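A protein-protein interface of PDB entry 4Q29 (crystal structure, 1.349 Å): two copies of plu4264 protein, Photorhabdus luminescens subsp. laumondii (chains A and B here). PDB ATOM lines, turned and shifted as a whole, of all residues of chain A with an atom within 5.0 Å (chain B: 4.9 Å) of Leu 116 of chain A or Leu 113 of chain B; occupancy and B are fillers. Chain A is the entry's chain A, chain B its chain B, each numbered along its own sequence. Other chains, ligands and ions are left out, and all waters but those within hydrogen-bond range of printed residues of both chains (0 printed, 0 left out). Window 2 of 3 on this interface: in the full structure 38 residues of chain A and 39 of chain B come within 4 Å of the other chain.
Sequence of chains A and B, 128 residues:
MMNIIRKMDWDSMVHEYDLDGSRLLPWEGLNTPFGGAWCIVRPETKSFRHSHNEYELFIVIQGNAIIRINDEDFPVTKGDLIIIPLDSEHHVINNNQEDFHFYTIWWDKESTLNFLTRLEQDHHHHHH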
ATOM      1  N   THR A 112     -17.180 -23.325 -26.504  1.00  0.00           N
ATOM      2  CA  THR A 112     -15.779 -23.566 -26.179  1.00  0.00           C
ATOM      3  C   THR A 112     -15.277 -22.502 -25.214  1.00  0.00           C
ATOM      4  O   THR A 112     -14.757 -22.835 -24.165  1.00  0.00           O
ATOM      5  CB  THR A 112     -14.859 -23.627 -27.394  1.00  0.00           C
ATOM      6  OG1 THR A 112     -14.211 -22.345 -27.545  1.00  0.00           O
ATOM      7  CG2 THR A 112     -15.581 -24.100 -28.660  1.00  0.00           C
ATOM      8  N   LEU A 113     -15.432 -21.244 -25.592  1.00  0.00           N
ATOM      9  CA  LEU A 113     -15.057 -20.160 -24.689  1.00  0.00           C
ATOM     10  C   LEU A 113     -15.766 -20.284 -23.357  1.00  0.00           C
ATOM     11  O   LEU A 113     -15.180 -20.036 -22.314  1.00  0.00           O
ATOM     12  CB  LEU A 113     -15.355 -18.789 -25.317  1.00  0.00           C
ATOM     13  CG  LEU A 113     -14.421 -18.343 -26.444  1.00  0.00           C
ATOM     14  CD1 LEU A 113     -14.900 -17.036 -27.100  1.00  0.00           C
ATOM     15  CD2 LEU A 113     -12.949 -18.235 -25.947  1.00  0.00           C
ATOM     16  N   ASN A 114     -17.016 -20.738 -23.352  1.00  0.00           N
ATOM     17  CA  ASN A 114     -17.684 -20.876 -22.065  1.00  0.00           C
ATOM     18  C   ASN A 114     -17.023 -22.000 -21.237  1.00  0.00           C
ATOM     19  O   ASN A 114     -16.932 -21.904 -20.015  1.00  0.00           O
ATOM     20  CB  ASN A 114     -19.209 -21.057 -22.230  1.00  0.00           C
ATOM     21  CG  ASN A 114     -19.990 -19.703 -22.491  1.00  0.00           C
ATOM     22  OD1 ASN A 114     -19.450 -18.642 -22.944  1.00  0.00           O
ATOM     23  ND2 ASN A 114     -21.286 -19.751 -22.189  1.00  0.00           N
ATOM     24  N   PHE A 115     -16.571 -23.078 -21.909  1.00  0.00           N
ATOM     25  CA  PHE A 115     -15.817 -24.125 -21.235  1.00  0.00           C
ATOM     26  C   PHE A 115     -14.500 -23.611 -20.573  1.00  0.00           C
ATOM     27  O   PHE A 115     -14.174 -23.960 -19.457  1.00  0.00           O
ATOM     28  CB  PHE A 115     -15.593 -25.333 -22.208  1.00  0.00           C
ATOM     29  CG  PHE A 115     -14.452 -26.213 -21.808  1.00  0.00           C
ATOM     30  CD1 PHE A 115     -14.682 -27.214 -20.869  1.00  0.00           C
ATOM     31  CD2 PHE A 115     -13.190 -26.114 -22.361  1.00  0.00           C
ATOM     32  CE1 PHE A 115     -13.678 -28.024 -20.463  1.00  0.00           C
ATOM     33  CE2 PHE A 115     -12.169 -26.901 -21.942  1.00  0.00           C
ATOM     34  CZ  PHE A 115     -12.418 -27.896 -21.014  1.00  0.00           C
ATOM     35  N   LEU A 116     -13.756 -22.847 -21.360  1.00  0.00           N
ATOM     36  CA  LEU A 116     -12.510 -22.250 -20.846  1.00  0.00           C
ATOM     37  C   LEU A 116     -12.725 -21.280 -19.669  1.00  0.00           C
ATOM     38  O   LEU A 116     -12.006 -21.370 -18.685  1.00  0.00           O
ATOM     39  CB  LEU A 116     -11.801 -21.540 -21.985  1.00  0.00           C
ATOM     40  CG  LEU A 116     -11.334 -22.378 -23.172  1.00  0.00           C
ATOM     41  CD1 LEU A 116     -10.719 -21.572 -24.322  1.00  0.00           C
ATOM     42  CD2 LEU A 116     -10.381 -23.462 -22.714  1.00  0.00           C
ATOM     43  N   THR A 117     -13.797 -20.513 -19.738  1.00  0.00           N
ATOM     44  CA  THR A 117     -14.117 -19.568 -18.662  1.00  0.00           C
ATOM     45  C   THR A 117     -14.395 -20.343 -17.373  1.00  0.00           C
ATOM     46  O   THR A 117     -13.993 -19.970 -16.292  1.00  0.00           O
ATOM     47  CB  THR A 117     -15.314 -18.623 -19.031  1.00  0.00           C
ATOM     48  OG1 THR A 117     -14.879 -17.631 -19.985  1.00  0.00           O
ATOM     49  CG2 THR A 117     -15.844 -17.913 -17.792  1.00  0.00           C
ATOM     50  N   ARG A 118     -15.055 -21.499 -17.510  1.00  0.00           N
ATOM     51  CA  ARG A 118     -15.365 -22.338 -16.354  1.00  0.00           C
ATOM     52  C   ARG A 118     -14.185 -23.010 -15.654  1.00  0.00           C
ATOM     53  O   ARG A 118     -14.164 -23.051 -14.434  1.00  0.00           O
ATOM     54  CB  ARG A 118     -16.396 -23.392 -16.747  1.00  0.00           C
ATOM     55  CG  ARG A 118     -17.762 -22.792 -16.877  1.00  0.00           C
ATOM     56  CD  ARG A 118     -18.804 -23.851 -17.141  1.00  0.00           C
ATOM     57  NE  ARG A 118     -18.607 -24.430 -18.466  1.00  0.00           N
ATOM     58  CZ  ARG A 118     -19.491 -25.118 -19.186  1.00  0.00           C
ATOM     59  NH1 ARG A 118     -20.716 -25.445 -18.747  1.00  0.00           N
ATOM     60  NH2 ARG A 118     -19.110 -25.526 -20.374  1.00  0.00           N
ATOM     61  N   LEU A 119     -13.201 -23.515 -16.388  1.00  0.00           N
ATOM     62  CA  LEU A 119     -12.018 -24.057 -15.728  1.00  0.00           C
ATOM     63  C   LEU A 119     -11.407 -22.907 -14.934  1.00  0.00           C
ATOM     64  O   LEU A 119     -10.975 -23.076 -13.806  1.00  0.00           O
ATOM     65  CB  LEU A 119     -10.915 -24.539 -16.674  1.00  0.00           C
ATOM     66  CG  LEU A 119     -11.053 -25.536 -17.805  1.00  0.00           C
ATOM     67  CD1 LEU A 119      -9.858 -25.371 -18.714  1.00  0.00           C
ATOM     68  CD2 LEU A 119     -11.101 -26.952 -17.244  1.00  0.00           C
ATOM     69  N   GLU A 120     -11.342 -21.734 -15.564  1.00  0.00           N
ATOM     70  CA  GLU A 120     -10.679 -20.596 -14.938  1.00  0.00           C
ATOM     71  C   GLU A 120     -11.411 -20.186 -13.663  1.00  0.00           C
ATOM     72  O   GLU A 120     -10.786 -19.723 -12.709  1.00  0.00           O
ATOM     73  CB  GLU A 120     -10.587 -19.406 -15.897  1.00  0.00           C
ATOM     74  CG  GLU A 120      -9.513 -18.370 -15.535  1.00  0.00           C
ATOM     75  CD  GLU A 120      -8.109 -18.972 -15.456  1.00  0.00           C
ATOM     76  OE1 GLU A 120      -7.229 -18.368 -14.788  1.00  0.00           O
ATOM     77  OE2 GLU A 120      -7.895 -20.054 -16.062  1.00  0.00           O
ATOM     78  N   LYS B 109      -7.890 -28.231 -22.384  1.00  0.00           N
ATOM     79  CA  LYS B 109      -7.583 -26.817 -22.644  1.00  0.00           C
ATOM     80  C   LYS B 109      -6.951 -26.668 -24.009  1.00  0.00           C
ATOM     81  O   LYS B 109      -7.399 -25.850 -24.825  1.00  0.00           O
ATOM     82  CB  LYS B 109      -6.633 -26.288 -21.555  1.00  0.00           C
ATOM     83  CG  LYS B 109      -7.275 -26.048 -20.183  1.00  0.00           C
ATOM     84  CD  LYS B 109      -6.270 -25.872 -18.996  1.00  0.00           C
ATOM     85  CE  LYS B 109      -5.867 -27.215 -18.337  1.00  0.00           C
ATOM     86  NZ  LYS B 109      -4.721 -27.083 -17.380  1.00  0.00           N
ATOM     87  N   GLU B 110      -5.945 -27.489 -24.279  1.00  0.00           N
ATOM     88  CA  GLU B 110      -5.231 -27.440 -25.552  1.00  0.00           C
ATOM     89  C   GLU B 110      -6.139 -27.641 -26.741  1.00  0.00           C
ATOM     90  O   GLU B 110      -6.102 -26.913 -27.722  1.00  0.00           O
ATOM     91  CB  GLU B 110      -4.117 -28.497 -25.611  1.00  0.00           C
ATOM     92  CG  GLU B 110      -3.625 -28.768 -27.052  1.00  0.00           C
ATOM     93  CD  GLU B 110      -2.449 -29.727 -27.121  1.00  0.00           C
ATOM     94  OE1 GLU B 110      -1.653 -29.755 -26.179  1.00  0.00           O
ATOM     95  OE2 GLU B 110      -2.359 -30.483 -28.121  1.00  0.00           O
ATOM     96  N   SER B 111      -6.962 -28.682 -26.670  1.00  0.00           N
ATOM     97  CA  SER B 111      -7.780 -29.030 -27.852  1.00  0.00           C
ATOM     98  C   SER B 111      -8.793 -27.923 -28.127  1.00  0.00           C
ATOM     99  O   SER B 111      -9.130 -27.656 -29.263  1.00  0.00           O
ATOM    100  CB  SER B 111      -8.443 -30.410 -27.723  1.00  0.00           C
ATOM    101  OG  SER B 111      -9.386 -30.435 -26.695  1.00  0.00           O
ATOM    102  N   THR B 112      -9.302 -27.327 -27.064  1.00  0.00           N
ATOM    103  CA  THR B 112     -10.292 -26.265 -27.171  1.00  0.00           C
ATOM    104  C   THR B 112      -9.655 -24.974 -27.732  1.00  0.00           C
ATOM    105  O   THR B 112     -10.174 -24.412 -28.689  1.00  0.00           O
ATOM    106  CB  THR B 112     -11.014 -26.075 -25.822  1.00  0.00           C
ATOM    107  OG1 THR B 112     -11.499 -27.345 -25.366  1.00  0.00           O
ATOM    108  CG2 THR B 112     -12.199 -25.158 -25.939  1.00  0.00           C
ATOM    109  N   LEU B 113      -8.522 -24.569 -27.168  1.00  0.00           N
ATOM    110  CA  LEU B 113      -7.813 -23.413 -27.690  1.00  0.00           C
ATOM    111  C   LEU B 113      -7.424 -23.632 -29.143  1.00  0.00           C
ATOM    112  O   LEU B 113      -7.520 -22.704 -29.963  1.00  0.00           O
ATOM    113  CB  LEU B 113      -6.554 -23.091 -26.869  1.00  0.00           C
ATOM    114  CG  LEU B 113      -6.626 -22.519 -25.454  1.00  0.00           C
ATOM    115  CD1 LEU B 113      -5.197 -22.450 -24.856  1.00  0.00           C
ATOM    116  CD2 LEU B 113      -7.277 -21.125 -25.440  1.00  0.00           C
ATOM    117  N   ASN B 114      -6.964 -24.843 -29.465  1.00  0.00           N
ATOM    118  CA  ASN B 114      -6.518 -25.119 -30.811  1.00  0.00           C
ATOM    119  C   ASN B 114      -7.703 -24.975 -31.778  1.00  0.00           C
ATOM    120  O   ASN B 114      -7.554 -24.492 -32.870  1.00  0.00           O
ATOM    121  CB  ASN B 114      -5.881 -26.512 -30.915  1.00  0.00           C
ATOM    122  CG  ASN B 114      -4.440 -26.579 -30.326  1.00  0.00           C
ATOM    123  OD1 ASN B 114      -3.788 -27.610 -30.448  1.00  0.00           O
ATOM    124  ND2 ASN B 114      -3.934 -25.477 -29.735  1.00  0.00           N
ATOM    125  N   PHE B 115      -8.900 -25.448 -31.405  1.00  0.00           N
ATOM    126  CA  PHE B 115     -10.074 -25.173 -32.222  1.00  0.00           C
ATOM    127  C   PHE B 115     -10.321 -23.655 -32.507  1.00  0.00           C
ATOM    128  O   PHE B 115     -10.603 -23.257 -33.619  1.00  0.00           O
ATOM    129  CB  PHE B 115     -11.309 -25.837 -31.563  1.00  0.00           C
ATOM    130  CG  PHE B 115     -12.591 -25.278 -32.028  1.00  0.00           C
ATOM    131  CD1 PHE B 115     -13.137 -25.734 -33.248  1.00  0.00           C
ATOM    132  CD2 PHE B 115     -13.303 -24.352 -31.286  1.00  0.00           C
ATOM    133  CE1 PHE B 115     -14.325 -25.206 -33.720  1.00  0.00           C
ATOM    134  CE2 PHE B 115     -14.458 -23.822 -31.738  1.00  0.00           C
ATOM    135  CZ  PHE B 115     -15.011 -24.271 -32.953  1.00  0.00           C
ATOM    136  N   LEU B 116     -10.250 -22.876 -31.436  1.00  0.00           N
ATOM    137  CA  LEU B 116     -10.421 -21.421 -31.559  1.00  0.00           C
ATOM    138  C   LEU B 116      -9.377 -20.714 -32.445  1.00  0.00           C
ATOM    139  O   LEU B 116      -9.738 -19.895 -33.248  1.00  0.00           O
ATOM    140  CB  LEU B 116     -10.359 -20.881 -30.157  1.00  0.00           C
ATOM    141  CG  LEU B 116     -11.617 -20.930 -29.290  1.00  0.00           C
ATOM    142  CD1 LEU B 116     -11.241 -20.878 -27.811  1.00  0.00           C
ATOM    143  CD2 LEU B 116     -12.447 -19.683 -29.640  1.00  0.00           C
ATOM    144  N   THR B 117      -8.161 -21.212 -32.380  1.00  0.00           N
ATOM    145  CA  THR B 117      -7.080 -20.684 -33.195  1.00  0.00           C
ATOM    146  C   THR B 117      -7.298 -20.946 -34.675  1.00  0.00           C
ATOM    147  O   THR B 117      -7.152 -20.066 -35.503  1.00  0.00           O
ATOM    148  CB  THR B 117      -5.753 -21.222 -32.674  1.00  0.00           C
ATOM    149  OG1 THR B 117      -5.594 -20.764 -31.320  1.00  0.00           O
ATOM    150  CG2 THR B 117      -4.586 -20.743 -33.535  1.00  0.00           C
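The side-chain hydroxyl (OG1) of Thr 117 of chain A sits at hydrogen-bond distance from the backbone carbonyl oxygen (O) of Leu 113 of chain A.
The side-chain hydroxyl (OG1) of Thr 117 of chain B lies within hydrogen-bond range of the backbone carbonyl oxygen (O) of Leu 113 of chain B, 3.1 Å away.
Among the printed residues, merely in contact across the chains: Thr 112 of chain A with Thr 112 of chain B, Thr 112 of chain A with Phe 115 of chain B, Thr 112 of chain A with Leu 116 of chain B, Leu 113 of chain A with Leu 116 of chain B, Phe 115 of chain A with Thr 112 of chain B, Leu 116 of chain A with Leu 113 of chain B, Leu 116 of chain A with Leu 116 of chain B and Leu 119 of chain A with Lys 109 of chain B.
Of the printed residues of chain B, Phe 115 of chain A touches Thr 112 (3.5 Å).
Thr 117 of chain A touches none of the printed residues of chain B.
Of the printed residues of chain B, Leu 119 of chain A touches Lys 109.
Of the printed residues of chain A, Thr 112 of chain B touches Thr 112 and Phe 115.
Of chain A, only Leu 116 comes within 4 Å of Leu 113 of chain B.
Asn 114 of chain B touches none of the printed residues of chain A.
Printed residues of chain A within 4 Å of Phe 115 of chain B: Thr 112 (3.3 Å).
The nearest printed residue of chain B that does not touch Leu 119 of chain A is Glu 110 of chain B (7.1 Å).
Hydrophobic or aromatic side chains of chain A within 4 Å of the printed part of chain B: Leu 113, Phe 115, Leu 116 and Leu 119.
Among the printed residues, 8 pairs touch across the chains.
Thr 112 of chain B touches its own counterpart, Thr 112 of chain A.
Thr 112 of chain A touches Phe 115 of chain B, and with the chains exchanged Phe 115 of chain A touches Thr 112 of chain B.
Thr 112 of chain A touches Leu 116 of chain B, but with the chains exchanged Leu 116 of chain A does not touch Thr 112 of chain B (4.02 Å).
Leu 113 of chain A touches Leu 116 of chain B, and with the chains exchanged Leu 116 of chain A touches Leu 113 of chain B.
Positions printed for both chains: 112, 113, 114, 115, 116 and 117.
Of the 8 pairs that touch across the chains among the printed residues, 6 have their exchanged pair printed and touching as well.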
